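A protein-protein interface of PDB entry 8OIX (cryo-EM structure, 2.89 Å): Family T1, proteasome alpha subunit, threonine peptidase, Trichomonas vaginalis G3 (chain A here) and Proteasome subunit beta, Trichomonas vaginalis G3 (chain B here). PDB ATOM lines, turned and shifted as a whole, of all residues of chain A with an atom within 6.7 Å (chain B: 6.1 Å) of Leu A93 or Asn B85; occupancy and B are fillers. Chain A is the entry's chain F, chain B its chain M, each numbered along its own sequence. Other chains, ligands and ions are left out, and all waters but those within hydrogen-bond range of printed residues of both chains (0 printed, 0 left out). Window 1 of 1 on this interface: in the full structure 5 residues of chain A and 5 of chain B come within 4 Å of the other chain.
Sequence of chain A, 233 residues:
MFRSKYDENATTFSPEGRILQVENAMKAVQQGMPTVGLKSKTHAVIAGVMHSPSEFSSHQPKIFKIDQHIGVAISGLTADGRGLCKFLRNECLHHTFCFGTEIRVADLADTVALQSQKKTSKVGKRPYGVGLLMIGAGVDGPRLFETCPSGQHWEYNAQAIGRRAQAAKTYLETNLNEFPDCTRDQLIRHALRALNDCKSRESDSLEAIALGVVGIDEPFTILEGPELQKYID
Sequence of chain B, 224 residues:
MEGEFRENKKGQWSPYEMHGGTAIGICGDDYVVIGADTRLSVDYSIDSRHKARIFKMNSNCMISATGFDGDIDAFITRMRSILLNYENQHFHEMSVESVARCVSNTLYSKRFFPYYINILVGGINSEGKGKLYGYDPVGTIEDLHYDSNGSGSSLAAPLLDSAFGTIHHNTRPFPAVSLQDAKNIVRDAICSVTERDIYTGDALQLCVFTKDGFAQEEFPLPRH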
ATOM      1  N   ASP A  67       0.901  27.374  17.742  1.00  0.00           N
ATOM      2  CA  ASP A  67       1.059  28.648  18.429  1.00  0.00           C
ATOM      3  C   ASP A  67       1.463  29.719  17.425  1.00  0.00           C
ATOM      4  O   ASP A  67       1.636  29.420  16.238  1.00  0.00           O
ATOM      5  CB  ASP A  67       2.090  28.539  19.553  1.00  0.00           C
ATOM      6  CG  ASP A  67       1.754  29.426  20.735  1.00  0.00           C
ATOM      7  OD1 ASP A  67       1.044  30.434  20.540  1.00  0.00           O
ATOM      8  OD2 ASP A  67       2.203  29.121  21.859  1.00  0.00           O
ATOM      9  N   LEU A  88      -1.232  19.746  21.544  1.00  0.00           N
ATOM     10  CA  LEU A  88      -0.128  20.682  21.375  1.00  0.00           C
ATOM     11  C   LEU A  88      -0.553  22.105  21.705  1.00  0.00           C
ATOM     12  O   LEU A  88       0.224  22.870  22.281  1.00  0.00           O
ATOM     13  CB  LEU A  88       0.410  20.602  19.949  1.00  0.00           C
ATOM     14  CG  LEU A  88       1.101  19.303  19.542  1.00  0.00           C
ATOM     15  CD1 LEU A  88       1.388  19.325  18.055  1.00  0.00           C
ATOM     16  CD2 LEU A  88       2.378  19.096  20.336  1.00  0.00           C
ATOM     17  N   ARG A  89      -1.775  22.486  21.330  1.00  0.00           N
ATOM     18  CA  ARG A  89      -2.262  23.818  21.664  1.00  0.00           C
ATOM     19  C   ARG A  89      -2.480  23.961  23.163  1.00  0.00           C
ATOM     20  O   ARG A  89      -2.221  25.025  23.731  1.00  0.00           O
ATOM     21  CB  ARG A  89      -3.541  24.112  20.887  1.00  0.00           C
ATOM     22  CG  ARG A  89      -3.284  24.415  19.424  1.00  0.00           C
ATOM     23  CD  ARG A  89      -4.523  24.206  18.582  1.00  0.00           C
ATOM     24  NE  ARG A  89      -4.251  24.447  17.171  1.00  0.00           N
ATOM     25  CZ  ARG A  89      -5.077  24.129  16.185  1.00  0.00           C
ATOM     26  NH1 ARG A  89      -6.241  23.548  16.419  1.00  0.00           N
ATOM     27  NH2 ARG A  89      -4.724  24.397  14.931  1.00  0.00           N
ATOM     28  N   ASN A  90      -2.928  22.893  23.827  1.00  0.00           N
ATOM     29  CA  ASN A  90      -3.008  22.923  25.285  1.00  0.00           C
ATOM     30  C   ASN A  90      -1.625  23.075  25.901  1.00  0.00           C
ATOM     31  O   ASN A  90      -1.449  23.806  26.881  1.00  0.00           O
ATOM     32  CB  ASN A  90      -3.695  21.662  25.810  1.00  0.00           C
ATOM     33  CG  ASN A  90      -5.096  21.490  25.261  1.00  0.00           C
ATOM     34  OD1 ASN A  90      -5.713  22.447  24.793  1.00  0.00           O
ATOM     35  ND2 ASN A  90      -5.605  20.265  25.314  1.00  0.00           N
ATOM     36  N   GLU A  91      -0.628  22.388  25.339  1.00  0.00           N
ATOM     37  CA  GLU A  91       0.727  22.501  25.868  1.00  0.00           C
ATOM     38  C   GLU A  91       1.279  23.905  25.648  1.00  0.00           C
ATOM     39  O   GLU A  91       1.950  24.462  26.526  1.00  0.00           O
ATOM     40  CB  GLU A  91       1.632  21.455  25.220  1.00  0.00           C
ATOM     41  CG  GLU A  91       1.353  20.033  25.669  1.00  0.00           C
ATOM     42  CD  GLU A  91       1.608  19.828  27.147  1.00  0.00           C
ATOM     43  OE1 GLU A  91       2.754  20.051  27.590  1.00  0.00           O
ATOM     44  OE2 GLU A  91       0.664  19.446  27.868  1.00  0.00           O
ATOM     45  N   CYS A  92       0.967  24.509  24.500  1.00  0.00           N
ATOM     46  CA  CYS A  92       1.414  25.870  24.237  1.00  0.00           C
ATOM     47  C   CYS A  92       0.694  26.858  25.135  1.00  0.00           C
ATOM     48  O   CYS A  92       1.285  27.851  25.564  1.00  0.00           O
ATOM     49  CB  CYS A  92       1.167  26.243  22.778  1.00  0.00           C
ATOM     50  SG  CYS A  92       2.194  25.389  21.601  1.00  0.00           S
ATOM     51  N   LEU A  93      -0.544  26.552  25.504  1.00  0.00           N
ATOM     52  CA  LEU A  93      -1.313  27.453  26.336  1.00  0.00           C
ATOM     53  C   LEU A  93      -0.926  27.315  27.795  1.00  0.00           C
ATOM     54  O   LEU A  93      -0.943  28.308  28.528  1.00  0.00           O
ATOM     55  CB  LEU A  93      -2.801  27.154  26.143  1.00  0.00           C
ATOM     56  CG  LEU A  93      -3.911  27.944  26.823  1.00  0.00           C
ATOM     57  CD1 LEU A  93      -5.071  28.033  25.854  1.00  0.00           C
ATOM     58  CD2 LEU A  93      -4.345  27.282  28.118  1.00  0.00           C
ATOM     59  N   HIS A  94      -0.383  26.165  28.176  1.00  0.00           N
ATOM     60  CA  HIS A  94       0.081  25.979  29.538  1.00  0.00           C
ATOM     61  C   HIS A  94       1.533  26.392  29.688  1.00  0.00           C
ATOM     62  O   HIS A  94       1.965  26.696  30.803  1.00  0.00           O
ATOM     63  CB  HIS A  94      -0.095  24.515  29.963  1.00  0.00           C
ATOM     64  CG  HIS A  94       0.245  24.255  31.396  1.00  0.00           C
ATOM     65  ND1 HIS A  94      -0.640  24.495  32.424  1.00  0.00           N
ATOM     66  CD2 HIS A  94       1.370  23.771  31.972  1.00  0.00           C
ATOM     67  CE1 HIS A  94      -0.074  24.173  33.574  1.00  0.00           C
ATOM     68  NE2 HIS A  94       1.146  23.732  33.327  1.00  0.00           N
ATOM     69  N   HIS A  95       2.256  26.527  28.578  1.00  0.00           N
ATOM     70  CA  HIS A  95       3.586  27.110  28.624  1.00  0.00           C
ATOM     71  C   HIS A  95       3.521  28.623  28.501  1.00  0.00           C
ATOM     72  O   HIS A  95       4.421  29.317  28.985  1.00  0.00           O
ATOM     73  CB  HIS A  95       4.466  26.538  27.513  1.00  0.00           C
ATOM     74  CG  HIS A  95       5.898  26.963  27.602  1.00  0.00           C
ATOM     75  ND1 HIS A  95       6.348  28.168  27.111  1.00  0.00           N
ATOM     76  CD2 HIS A  95       6.983  26.335  28.112  1.00  0.00           C
ATOM     77  CE1 HIS A  95       7.648  28.270  27.324  1.00  0.00           C
ATOM     78  NE2 HIS A  95       8.057  27.171  27.930  1.00  0.00           N
ATOM     79  N   THR A  96       2.468  29.145  27.869  1.00  0.00           N
ATOM     80  CA  THR A  96       2.241  30.578  27.797  1.00  0.00           C
ATOM     81  C   THR A  96       1.451  31.057  29.007  1.00  0.00           C
ATOM     82  O   THR A  96       1.328  32.266  29.231  1.00  0.00           O
ATOM     83  CB  THR A  96       1.505  30.919  26.490  1.00  0.00           C
ATOM     84  OG1 THR A  96       2.249  30.400  25.382  1.00  0.00           O
ATOM     85  CG2 THR A  96       1.375  32.421  26.294  1.00  0.00           C
ATOM     86  N   PHE A  97       0.960  30.123  29.821  1.00  0.00           N
ATOM     87  CA  PHE A  97       0.375  30.437  31.114  1.00  0.00           C
ATOM     88  C   PHE A  97       1.408  30.332  32.225  1.00  0.00           C
ATOM     89  O   PHE A  97       1.555  31.264  33.018  1.00  0.00           O
ATOM     90  CB  PHE A  97      -0.810  29.502  31.398  1.00  0.00           C
ATOM     91  CG  PHE A  97      -1.301  29.552  32.820  1.00  0.00           C
ATOM     92  CD1 PHE A  97      -2.255  30.477  33.204  1.00  0.00           C
ATOM     93  CD2 PHE A  97      -0.823  28.661  33.767  1.00  0.00           C
ATOM     94  CE1 PHE A  97      -2.713  30.523  34.504  1.00  0.00           C
ATOM     95  CE2 PHE A  97      -1.275  28.704  35.070  1.00  0.00           C
ATOM     96  CZ  PHE A  97      -2.222  29.636  35.437  1.00  0.00           C
ATOM     97  N   CYS A  98       2.146  29.221  32.290  1.00  0.00           N
ATOM     98  CA  CYS A  98       3.136  29.069  33.351  1.00  0.00           C
ATOM     99  C   CYS A  98       4.289  30.049  33.181  1.00  0.00           C
ATOM    100  O   CYS A  98       4.734  30.661  34.155  1.00  0.00           O
ATOM    101  CB  CYS A  98       3.655  27.633  33.395  1.00  0.00           C
ATOM    102  SG  CYS A  98       2.418  26.402  33.843  1.00  0.00           S
ATOM    103  N   ILE A 103       6.185  28.343  23.873  1.00  0.00           N
ATOM    104  CA  ILE A 103       6.968  27.129  24.039  1.00  0.00           C
ATOM    105  C   ILE A 103       7.845  26.907  22.811  1.00  0.00           C
ATOM    106  O   ILE A 103       7.575  27.407  21.713  1.00  0.00           O
ATOM    107  CB  ILE A 103       6.043  25.928  24.295  1.00  0.00           C
ATOM    108  CG1 ILE A 103       6.830  24.702  24.764  1.00  0.00           C
ATOM    109  CG2 ILE A 103       5.281  25.584  23.047  1.00  0.00           C
ATOM    110  CD1 ILE A 103       5.956  23.578  25.268  1.00  0.00           C
ATOM    111  N   ARG B  80      -7.164  35.436  27.205  1.00  0.00           N
ATOM    112  CA  ARG B  80      -6.275  35.183  26.081  1.00  0.00           C
ATOM    113  C   ARG B  80      -6.247  33.700  25.738  1.00  0.00           C
ATOM    114  O   ARG B  80      -6.242  33.330  24.560  1.00  0.00           O
ATOM    115  CB  ARG B  80      -4.876  35.708  26.395  1.00  0.00           C
ATOM    116  CG  ARG B  80      -4.781  37.215  26.282  1.00  0.00           C
ATOM    117  CD  ARG B  80      -3.488  37.758  26.852  1.00  0.00           C
ATOM    118  NE  ARG B  80      -3.370  39.190  26.605  1.00  0.00           N
ATOM    119  CZ  ARG B  80      -2.475  39.980  27.181  1.00  0.00           C
ATOM    120  NH1 ARG B  80      -1.610  39.514  28.065  1.00  0.00           N
ATOM    121  NH2 ARG B  80      -2.453  41.272  26.866  1.00  0.00           N
ATOM    122  N   SER B  81      -6.252  32.840  26.757  1.00  0.00           N
ATOM    123  CA  SER B  81      -6.325  31.404  26.520  1.00  0.00           C
ATOM    124  C   SER B  81      -7.609  31.027  25.795  1.00  0.00           C
ATOM    125  O   SER B  81      -7.585  30.243  24.840  1.00  0.00           O
ATOM    126  CB  SER B  81      -6.227  30.656  27.850  1.00  0.00           C
ATOM    127  OG  SER B  81      -4.907  30.691  28.361  1.00  0.00           O
ATOM    128  N   ILE B  82      -8.741  31.586  26.225  1.00  0.00           N
ATOM    129  CA  ILE B  82     -10.019  31.224  25.623  1.00  0.00           C
ATOM    130  C   ILE B  82     -10.119  31.774  24.208  1.00  0.00           C
ATOM    131  O   ILE B  82     -10.678  31.126  23.320  1.00  0.00           O
ATOM    132  CB  ILE B  82     -11.195  31.692  26.497  1.00  0.00           C
ATOM    133  CG1 ILE B  82     -11.133  31.035  27.873  1.00  0.00           C
ATOM    134  CG2 ILE B  82     -12.498  31.291  25.845  1.00  0.00           C
ATOM    135  CD1 ILE B  82     -11.904  31.782  28.936  1.00  0.00           C
ATOM    136  N   LEU B  83      -9.590  32.974  23.968  1.00  0.00           N
ATOM    137  CA  LEU B  83      -9.622  33.527  22.619  1.00  0.00           C
ATOM    138  C   LEU B  83      -8.699  32.759  21.686  1.00  0.00           C
ATOM    139  O   LEU B  83      -9.025  32.561  20.512  1.00  0.00           O
ATOM    140  CB  LEU B  83      -9.252  35.009  22.632  1.00  0.00           C
ATOM    141  CG  LEU B  83     -10.395  36.019  22.754  1.00  0.00           C
ATOM    142  CD1 LEU B  83     -11.181  35.849  24.037  1.00  0.00           C
ATOM    143  CD2 LEU B  83      -9.862  37.425  22.632  1.00  0.00           C
ATOM    144  N   LEU B  84      -7.545  32.314  22.183  1.00  0.00           N
ATOM    145  CA  LEU B  84      -6.682  31.463  21.373  1.00  0.00           C
ATOM    146  C   LEU B  84      -7.356  30.130  21.074  1.00  0.00           C
ATOM    147  O   LEU B  84      -7.282  29.628  19.946  1.00  0.00           O
ATOM    148  CB  LEU B  84      -5.349  31.251  22.087  1.00  0.00           C
ATOM    149  CG  LEU B  84      -4.155  30.886  21.211  1.00  0.00           C
ATOM    150  CD1 LEU B  84      -3.828  32.036  20.281  1.00  0.00           C
ATOM    151  CD2 LEU B  84      -2.956  30.532  22.072  1.00  0.00           C
ATOM    152  N   ASN B  85      -8.037  29.552  22.067  1.00  0.00           N
ATOM    153  CA  ASN B  85      -8.779  28.318  21.839  1.00  0.00           C
ATOM    154  C   ASN B  85      -9.896  28.527  20.827  1.00  0.00           C
ATOM    155  O   ASN B  85     -10.151  27.658  19.989  1.00  0.00           O
ATOM    156  CB  ASN B  85      -9.344  27.794  23.158  1.00  0.00           C
ATOM    157  CG  ASN B  85      -8.269  27.269  24.084  1.00  0.00           C
ATOM    158  OD1 ASN B  85      -7.238  26.769  23.634  1.00  0.00           O
ATOM    159  ND2 ASN B  85      -8.504  27.378  25.385  1.00  0.00           N
ATOM    160  N   TYR B  86     -10.588  29.662  20.906  1.00  0.00           N
ATOM    161  CA  TYR B  86     -11.638  29.968  19.944  1.00  0.00           C
ATOM    162  C   TYR B  86     -11.067  30.147  18.547  1.00  0.00           C
ATOM    163  O   TYR B  86     -11.682  29.732  17.563  1.00  0.00           O
ATOM    164  CB  TYR B  86     -12.396  31.219  20.379  1.00  0.00           C
ATOM    165  CG  TYR B  86     -13.524  31.625  19.457  1.00  0.00           C
ATOM    166  CD1 TYR B  86     -13.283  32.401  18.334  1.00  0.00           C
ATOM    167  CD2 TYR B  86     -14.830  31.239  19.717  1.00  0.00           C
ATOM    168  CE1 TYR B  86     -14.303  32.769  17.491  1.00  0.00           C
ATOM    169  CE2 TYR B  86     -15.860  31.610  18.880  1.00  0.00           C
ATOM    170  CZ  TYR B  86     -15.589  32.376  17.769  1.00  0.00           C
ATOM    171  OH  TYR B  86     -16.602  32.754  16.924  1.00  0.00           O
ATOM    172  N   GLU B  87      -9.910  30.796  18.434  1.00  0.00           N
ATOM    173  CA  GLU B  87      -9.288  30.953  17.127  1.00  0.00           C
ATOM    174  C   GLU B  87      -8.873  29.602  16.560  1.00  0.00           C
ATOM    175  O   GLU B  87      -8.940  29.381  15.345  1.00  0.00           O
ATOM    176  CB  GLU B  87      -8.091  31.896  17.231  1.00  0.00           C
ATOM    177  CG  GLU B  87      -7.662  32.507  15.909  1.00  0.00           C
ATOM    178  CD  GLU B  87      -6.723  33.683  16.093  1.00  0.00           C
ATOM    179  OE1 GLU B  87      -6.500  34.091  17.252  1.00  0.00           O
ATOM    180  OE2 GLU B  87      -6.210  34.202  15.079  1.00  0.00           O
ATOM    181  N   ASN B  88      -8.439  28.685  17.427  1.00  0.00           N
ATOM    182  CA  ASN B  88      -7.988  27.377  16.962  1.00  0.00           C
ATOM    183  C   ASN B  88      -9.152  26.455  16.610  1.00  0.00           C
ATOM    184  O   ASN B  88      -9.068  25.693  15.641  1.00  0.00           O
ATOM    185  CB  ASN B  88      -7.102  26.728  18.023  1.00  0.00           C
ATOM    186  CG  ASN B  88      -5.862  27.541  18.321  1.00  0.00           C
ATOM    187  OD1 ASN B  88      -5.369  28.278  17.468  1.00  0.00           O
ATOM    188  ND2 ASN B  88      -5.351  27.414  19.540  1.00  0.00           N
ATOM    189  N   GLN B  89     -10.238  26.505  17.382  1.00  0.00           N
ATOM    190  CA  GLN B  89     -11.344  25.566  17.237  1.00  0.00           C
ATOM    191  C   GLN B  89     -12.498  26.111  16.411  1.00  0.00           C
ATOM    192  O   GLN B  89     -13.339  25.326  15.958  1.00  0.00           O
ATOM    193  CB  GLN B  89     -11.874  25.158  18.617  1.00  0.00           C
ATOM    194  CG  GLN B  89     -10.817  24.592  19.545  1.00  0.00           C
ATOM    195  CD  GLN B  89     -11.381  24.195  20.892  1.00  0.00           C
ATOM    196  OE1 GLN B  89     -12.506  23.704  20.987  1.00  0.00           O
ATOM    197  NE2 GLN B  89     -10.603  24.410  21.946  1.00  0.00           N
ATOM    198  N   HIS B  90     -12.559  27.424  16.209  1.00  0.00           N
ATOM    199  CA  HIS B  90     -13.622  28.062  15.456  1.00  0.00           C
ATOM    200  C   HIS B  90     -13.086  28.927  14.327  1.00  0.00           C
ATOM    201  O   HIS B  90     -13.876  29.589  13.646  1.00  0.00           O
ATOM    202  CB  HIS B  90     -14.503  28.903  16.388  1.00  0.00           C
ATOM    203  CG  HIS B  90     -15.015  28.141  17.571  1.00  0.00           C
ATOM    204  ND1 HIS B  90     -14.353  28.111  18.778  1.00  0.00           N
ATOM    205  CD2 HIS B  90     -16.111  27.362  17.723  1.00  0.00           C
ATOM    206  CE1 HIS B  90     -15.026  27.356  19.628  1.00  0.00           C
ATOM    207  NE2 HIS B  90     -16.096  26.888  19.013  1.00  0.00           N
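Printed residues of chain A that touch a printed residue of chain B: Arg A89 and Leu A93.
Hydrophobic or aromatic side chains of chain A within 4 Å of the printed part of chain B: Leu A93.
Along chain B the printed residues that touch a printed residue of chain A span positions 81 to 88.
Among the printed residues, no Asp or Glu carboxylate lies within 4 Å of a Lys or Arg side-chain nitrogen of the other chain.
Among the printed residues, pairs that only touch across the chains: Arg A89 with Asn B88 (3.4 Å), Leu A93 with Ser B81 (3.3 Å) and Leu A93 with Asn B85 (3.3 Å).
The backbone carbonyl oxygen (O) of Leu B84 sits at hydrogen-bond distance from the side-chain amide nitrogen (ND2) of Asn B88, at 3.0 Å.
The backbone carbonyl oxygen (O) of Ser B81 lies within hydrogen-bond range of the side-chain amide nitrogen (ND2) of Asn B85, at 3.1 Å.
Leu A93 touches two residues of chain B.
Asn B85 touches just one residue of chain A: Leu A93 (3.3 Å).
Of the printed residues of chain B, Arg A89 touches Asn B88 (3.4 Å).
Printed residues of chain A within 4 Å of Asn B88: Arg A89 (3.4 Å).
Printed residues of chain A within 4 Å of Ser B81: Leu A93 (3.3 Å).
Ile B82 touches none of the printed residues of chain A.
The nearest printed residue of chain A that does not touch Asn B88 is Asp A67 (6.3 Å).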
